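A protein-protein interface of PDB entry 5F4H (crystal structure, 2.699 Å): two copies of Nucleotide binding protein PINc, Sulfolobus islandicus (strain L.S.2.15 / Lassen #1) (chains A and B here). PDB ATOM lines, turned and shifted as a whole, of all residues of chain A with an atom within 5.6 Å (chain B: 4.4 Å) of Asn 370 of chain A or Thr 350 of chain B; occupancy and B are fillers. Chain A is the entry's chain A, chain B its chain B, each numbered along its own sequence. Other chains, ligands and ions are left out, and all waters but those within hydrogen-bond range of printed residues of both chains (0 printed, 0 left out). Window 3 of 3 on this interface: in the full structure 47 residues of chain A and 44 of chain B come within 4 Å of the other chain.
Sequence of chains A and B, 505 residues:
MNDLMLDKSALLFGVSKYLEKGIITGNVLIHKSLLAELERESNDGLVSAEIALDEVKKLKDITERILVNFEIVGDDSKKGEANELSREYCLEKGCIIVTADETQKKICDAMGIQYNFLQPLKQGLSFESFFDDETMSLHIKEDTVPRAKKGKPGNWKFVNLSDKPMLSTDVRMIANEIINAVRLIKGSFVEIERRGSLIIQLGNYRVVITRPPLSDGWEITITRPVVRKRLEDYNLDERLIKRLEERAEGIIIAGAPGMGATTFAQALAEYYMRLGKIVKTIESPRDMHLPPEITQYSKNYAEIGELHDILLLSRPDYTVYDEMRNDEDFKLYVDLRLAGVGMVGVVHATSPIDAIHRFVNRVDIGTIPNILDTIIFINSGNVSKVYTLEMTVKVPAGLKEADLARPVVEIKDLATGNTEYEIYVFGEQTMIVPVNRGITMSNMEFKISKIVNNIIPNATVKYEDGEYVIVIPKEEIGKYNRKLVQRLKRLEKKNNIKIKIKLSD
The guanidinium group (NH1) of Arg 337 of chain A is in hydrogen-bond range of the backbone carbonyl oxygen (O) of Asn 370 of chain A (2.7 Å). The backbone carbonyl oxygen (O) of Ile 371 of chain A is in hydrogen-bond range of the guanidinium group (NE) of Arg 337 of chain A, at 3.0 Å. NH1 of Arg 337 of chain A is in salt-bridge range of OD1 of Asp 373 of chain A (3.8 Å).
Among the printed residues, merely in contact across the chains: Arg 337 of chain A with Pro 257 of chain B (3.7 Å), Gly 366 of chain A with Thr 350 of chain B (3.2 Å), Gly 366 of chain A with Asp 354 of chain B (3.9 Å), Thr 367 of chain A with Thr 350 of chain B (3.8 Å), Asn 370 of chain A with Ala 256 of chain B (3.98 Å), Asn 370 of chain A with Pro 257 of chain B (3.6 Å) and Asn 370 of chain A with Thr 350 of chain B (3.7 Å).
Of the 12 printed residues of chain A, 4 touch a printed residue of chain B. Printed residues of chain B that touch a printed residue of chain A: Ala 256, Pro 257, Thr 350 and Asp 354. Hydrophobic or aromatic side chains of chain B that line the printed part of chain A: Ala 256 and Pro 257. Along chain B the printed residues that touch a printed residue of chain A span positions 256 to 354. Among the printed residues, 7 pairs touch across the chains.
No position is printed for both chains.
Of chain B, only Ala 256, Pro 257 and Thr 350 come within 4 Å of Asn 370 of chain A. Of chain A, only Gly 366, Thr 367 and Asn 370 come within 4 Å of Thr 350 of chain B. Of the printed residues of chain A, Pro 257 of chain B touches Arg 337 and Asn 370. Printed residues of chain A within 4 Å of Asp 354 of chain B: Gly 366. Printed residues of chain B within 4 Å of Arg 337 of chain A: Pro 257 (3.7 Å). Printed residues of chain B within 4 Å of Gly 366 of chain A: Thr 350 (3.2 Å) and Asp 354 (3.9 Å). Printed residues of chain B within 4 Å of Thr 367 of chain A: Thr 350. The nearest printed residue of chain B that does not touch Asn 370 of chain A is Ala 349 of chain B (6.3 Å). The nearest residue of chain A that does not touch Thr 350 of chain B is Met 391 of chain A (4.8 Å). The nearest printed residue of chain B that does not touch Arg 337 of chain A is Ala 256 of chain B (7.2 Å).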
ATOM      1  N   GLY A 250      -6.714  33.011  -6.012  1.00  0.00           N
ATOM      2  CA  GLY A 250      -7.341  33.113  -7.289  1.00  0.00           C
ATOM      3  C   GLY A 250      -8.816  33.197  -7.060  1.00  0.00           C
ATOM      4  O   GLY A 250      -9.484  32.178  -6.764  1.00  0.00           O
ATOM      5  N   ARG A 337      -1.875  33.944 -12.825  1.00  0.00           N
ATOM      6  CA  ARG A 337      -2.017  32.996 -11.748  1.00  0.00           C
ATOM      7  C   ARG A 337      -0.856  32.039 -11.721  1.00  0.00           C
ATOM      8  O   ARG A 337      -0.359  31.692 -10.641  1.00  0.00           O
ATOM      9  CB  ARG A 337      -3.327  32.215 -11.875  1.00  0.00           C
ATOM     10  CG  ARG A 337      -4.563  32.975 -11.472  1.00  0.00           C
ATOM     11  CD  ARG A 337      -4.520  33.449 -10.035  1.00  0.00           C
ATOM     12  NE  ARG A 337      -4.530  32.348  -9.078  1.00  0.00           N
ATOM     13  CZ  ARG A 337      -3.657  32.165  -8.094  1.00  0.00           C
ATOM     14  NH1 ARG A 337      -3.821  31.133  -7.296  1.00  0.00           N
ATOM     15  NH2 ARG A 337      -2.637  33.000  -7.885  1.00  0.00           N
ATOM     16  N   ILE A 365      -6.591  19.665 -15.249  1.00  0.00           N
ATOM     17  CA  ILE A 365      -7.443  19.452 -14.077  1.00  0.00           C
ATOM     18  C   ILE A 365      -6.709  19.580 -12.770  1.00  0.00           C
ATOM     19  O   ILE A 365      -7.184  20.251 -11.870  1.00  0.00           O
ATOM     20  CB  ILE A 365      -8.045  18.043 -14.076  1.00  0.00           C
ATOM     21  CG1 ILE A 365      -8.761  17.791 -15.400  1.00  0.00           C
ATOM     22  CG2 ILE A 365      -8.967  17.835 -12.886  1.00  0.00           C
ATOM     23  CD1 ILE A 365     -10.141  18.409 -15.513  1.00  0.00           C
ATOM     24  N   GLY A 366      -5.561  18.931 -12.665  1.00  0.00           N
ATOM     25  CA  GLY A 366      -4.757  19.012 -11.451  1.00  0.00           C
ATOM     26  C   GLY A 366      -4.368  20.446 -11.148  1.00  0.00           C
ATOM     27  O   GLY A 366      -4.239  20.798  -9.970  1.00  0.00           O
ATOM     28  N   THR A 367      -4.173  21.242 -12.233  1.00  0.00           N
ATOM     29  CA  THR A 367      -3.818  22.688 -12.193  1.00  0.00           C
ATOM     30  C   THR A 367      -4.968  23.660 -11.807  1.00  0.00           C
ATOM     31  O   THR A 367      -4.708  24.738 -11.324  1.00  0.00           O
ATOM     32  CB  THR A 367      -3.180  23.162 -13.554  1.00  0.00           C
ATOM     33  N   ILE A 368      -6.225  23.267 -11.999  1.00  0.00           N
ATOM     34  CA  ILE A 368      -7.385  24.173 -11.806  1.00  0.00           C
ATOM     35  C   ILE A 368      -7.442  24.828 -10.446  1.00  0.00           C
ATOM     36  O   ILE A 368      -7.661  26.011 -10.353  1.00  0.00           O
ATOM     37  CB  ILE A 368      -8.741  23.472 -12.074  1.00  0.00           C
ATOM     38  CG1 ILE A 368      -8.791  23.043 -13.559  1.00  0.00           C
ATOM     39  CG2 ILE A 368      -9.924  24.377 -11.736  1.00  0.00           C
ATOM     40  CD1 ILE A 368     -10.133  22.566 -14.077  1.00  0.00           C
ATOM     41  N   PRO A 369      -7.274  24.067  -9.386  1.00  0.00           N
ATOM     42  CA  PRO A 369      -7.239  24.652  -8.058  1.00  0.00           C
ATOM     43  C   PRO A 369      -6.179  25.708  -7.883  1.00  0.00           C
ATOM     44  O   PRO A 369      -6.350  26.623  -7.090  1.00  0.00           O
ATOM     45  CB  PRO A 369      -6.889  23.483  -7.140  1.00  0.00           C
ATOM     46  CG  PRO A 369      -7.313  22.279  -7.892  1.00  0.00           C
ATOM     47  CD  PRO A 369      -7.227  22.601  -9.345  1.00  0.00           C
ATOM     48  N   ASN A 370      -5.071  25.573  -8.591  1.00  0.00           N
ATOM     49  CA  ASN A 370      -4.065  26.626  -8.588  1.00  0.00           C
ATOM     50  C   ASN A 370      -4.494  27.931  -9.295  1.00  0.00           C
ATOM     51  O   ASN A 370      -4.053  29.023  -8.958  1.00  0.00           O
ATOM     52  CB  ASN A 370      -2.779  26.132  -9.228  1.00  0.00           C
ATOM     53  CG  ASN A 370      -2.054  25.147  -8.383  1.00  0.00           C
ATOM     54  OD1 ASN A 370      -1.926  23.992  -8.758  1.00  0.00           O
ATOM     55  ND2 ASN A 370      -1.549  25.588  -7.254  1.00  0.00           N
ATOM     56  N   ILE A 371      -5.326  27.810 -10.314  1.00  0.00           N
ATOM     57  CA  ILE A 371      -5.897  28.967 -10.973  1.00  0.00           C
ATOM     58  C   ILE A 371      -6.989  29.606 -10.144  1.00  0.00           C
ATOM     59  O   ILE A 371      -6.976  30.815  -9.970  1.00  0.00           O
ATOM     60  CB  ILE A 371      -6.461  28.576 -12.340  1.00  0.00           C
ATOM     61  CG1 ILE A 371      -5.364  27.917 -13.181  1.00  0.00           C
ATOM     62  CG2 ILE A 371      -7.079  29.793 -13.037  1.00  0.00           C
ATOM     63  CD1 ILE A 371      -4.206  28.819 -13.460  1.00  0.00           C
ATOM     64  N   LEU A 372      -7.930  28.786  -9.669  1.00  0.00           N
ATOM     65  CA  LEU A 372      -9.093  29.230  -8.908  1.00  0.00           C
ATOM     66  C   LEU A 372      -9.238  28.565  -7.576  1.00  0.00           C
ATOM     67  O   LEU A 372      -9.309  27.349  -7.511  1.00  0.00           O
ATOM     68  CB  LEU A 372     -10.350  28.825  -9.630  1.00  0.00           C
ATOM     69  CG  LEU A 372     -10.473  29.335 -11.025  1.00  0.00           C
ATOM     70  CD1 LEU A 372     -11.528  28.611 -11.799  1.00  0.00           C
ATOM     71  CD2 LEU A 372     -10.794  30.781 -11.015  1.00  0.00           C
ATOM     72  N   ASP A 373      -9.341  29.345  -6.512  1.00  0.00           N
ATOM     73  CA  ASP A 373      -9.518  28.760  -5.204  1.00  0.00           C
ATOM     74  C   ASP A 373     -10.816  29.078  -4.572  1.00  0.00           C
ATOM     75  O   ASP A 373     -11.299  28.297  -3.770  1.00  0.00           O
ATOM     76  CB  ASP A 373      -8.603  29.406  -4.231  1.00  0.00           C
ATOM     77  CG  ASP A 373      -7.300  29.775  -4.820  1.00  0.00           C
ATOM     78  OD1 ASP A 373      -6.655  29.107  -5.745  1.00  0.00           O
ATOM     79  OD2 ASP A 373      -6.908  30.806  -4.283  1.00  0.00           O
ATOM     80  N   MET A 391      -8.194  20.008  -4.734  1.00  0.00           N
ATOM     81  CA  MET A 391      -7.882  18.948  -5.647  1.00  0.00           C
ATOM     82  C   MET A 391      -7.571  17.716  -4.854  1.00  0.00           C
ATOM     83  O   MET A 391      -6.780  17.742  -3.929  1.00  0.00           O
ATOM     84  CB  MET A 391      -6.706  19.297  -6.499  1.00  0.00           C
ATOM     85  CG  MET A 391      -6.479  18.317  -7.655  1.00  0.00           C
ATOM     86  SD  MET A 391      -5.236  17.046  -7.287  1.00  0.00           S
ATOM     87  CE  MET A 391      -5.012  16.174  -8.848  1.00  0.00           C
ATOM     88  N   ALA B 256       3.822  23.319  -9.225  1.00  0.00           N
ATOM     89  CA  ALA B 256       2.731  24.208  -9.039  1.00  0.00           C
ATOM     90  C   ALA B 256       3.245  25.654  -9.041  1.00  0.00           C
ATOM     91  O   ALA B 256       4.442  25.925  -8.852  1.00  0.00           O
ATOM     92  CB  ALA B 256       2.010  23.889  -7.761  1.00  0.00           C
ATOM     93  N   PRO B 257       2.335  26.614  -9.268  1.00  0.00           N
ATOM     94  CA  PRO B 257       2.871  27.964  -9.248  1.00  0.00           C
ATOM     95  C   PRO B 257       3.378  28.357  -7.879  1.00  0.00           C
ATOM     96  O   PRO B 257       2.806  27.945  -6.877  1.00  0.00           O
ATOM     97  CB  PRO B 257       1.662  28.802  -9.620  1.00  0.00           C
ATOM     98  CG  PRO B 257       0.850  27.896 -10.475  1.00  0.00           C
ATOM     99  CD  PRO B 257       0.936  26.605  -9.733  1.00  0.00           C
ATOM    100  N   ALA B 349       2.698  22.497 -13.817  1.00  0.00           N
ATOM    101  CA  ALA B 349       1.718  21.411 -13.823  1.00  0.00           C
ATOM    102  C   ALA B 349       1.843  20.623 -12.516  1.00  0.00           C
ATOM    103  O   ALA B 349       2.865  20.711 -11.851  1.00  0.00           O
ATOM    104  CB  ALA B 349       1.975  20.501 -15.003  1.00  0.00           C
ATOM    105  N   THR B 350       0.795  19.881 -12.159  1.00  0.00           N
ATOM    106  CA  THR B 350       0.795  19.028 -10.955  1.00  0.00           C
ATOM    107  C   THR B 350       1.008  17.529 -11.239  1.00  0.00           C
ATOM    108  O   THR B 350       1.360  16.781 -10.345  1.00  0.00           O
ATOM    109  CB  THR B 350      -0.527  19.211 -10.195  1.00  0.00           C
ATOM    110  OG1 THR B 350      -1.606  18.724 -11.001  1.00  0.00           O
ATOM    111  CG2 THR B 350      -0.766  20.678  -9.884  1.00  0.00           C
ATOM    112  N   SER B 351       0.858  17.123 -12.495  1.00  0.00           N
ATOM    113  CA  SER B 351       0.892  15.727 -12.894  1.00  0.00           C
ATOM    114  C   SER B 351       1.915  15.552 -14.016  1.00  0.00           C
ATOM    115  O   SER B 351       2.107  16.445 -14.804  1.00  0.00           O
ATOM    116  CB  SER B 351      -0.476  15.327 -13.418  1.00  0.00           C
ATOM    117  OG  SER B 351      -0.845  13.984 -13.175  1.00  0.00           O
ATOM    118  N   ASP B 354      -0.001  15.669 -17.288  1.00  0.00           N
ATOM    119  CA  ASP B 354      -0.347  17.081 -17.521  1.00  0.00           C
ATOM    120  C   ASP B 354       0.873  17.894 -18.046  1.00  0.00           C
ATOM    121  O   ASP B 354       0.730  18.644 -19.006  1.00  0.00           O
ATOM    122  CB  ASP B 354      -0.980  17.733 -16.266  1.00  0.00           C
ATOM    123  CG  ASP B 354      -2.349  17.101 -15.864  1.00  0.00           C
ATOM    124  OD1 ASP B 354      -3.096  16.593 -16.743  1.00  0.00           O
ATOM    125  OD2 ASP B 354      -2.679  17.129 -14.651  1.00  0.00           O
ATOM    126  N   PHE B 377      10.016  17.397 -10.738  1.00  0.00           N
ATOM    127  CA  PHE B 377       8.922  18.087 -10.034  1.00  0.00           C
ATOM    128  C   PHE B 377       9.487  18.903  -8.918  1.00  0.00           C
ATOM    129  O   PHE B 377      10.271  18.411  -8.106  1.00  0.00           O
ATOM    130  CB  PHE B 377       7.860  17.143  -9.448  1.00  0.00           C
ATOM    131  CG  PHE B 377       6.802  16.752 -10.433  1.00  0.00           C
ATOM    132  CD1 PHE B 377       7.110  15.846 -11.435  1.00  0.00           C
ATOM    133  CD2 PHE B 377       5.506  17.293 -10.400  1.00  0.00           C
ATOM    134  CE1 PHE B 377       6.140  15.470 -12.375  1.00  0.00           C
ATOM    135  CE2 PHE B 377       4.544  16.900 -11.337  1.00  0.00           C
ATOM    136  CZ  PHE B 377       4.872  15.997 -12.322  1.00  0.00           C
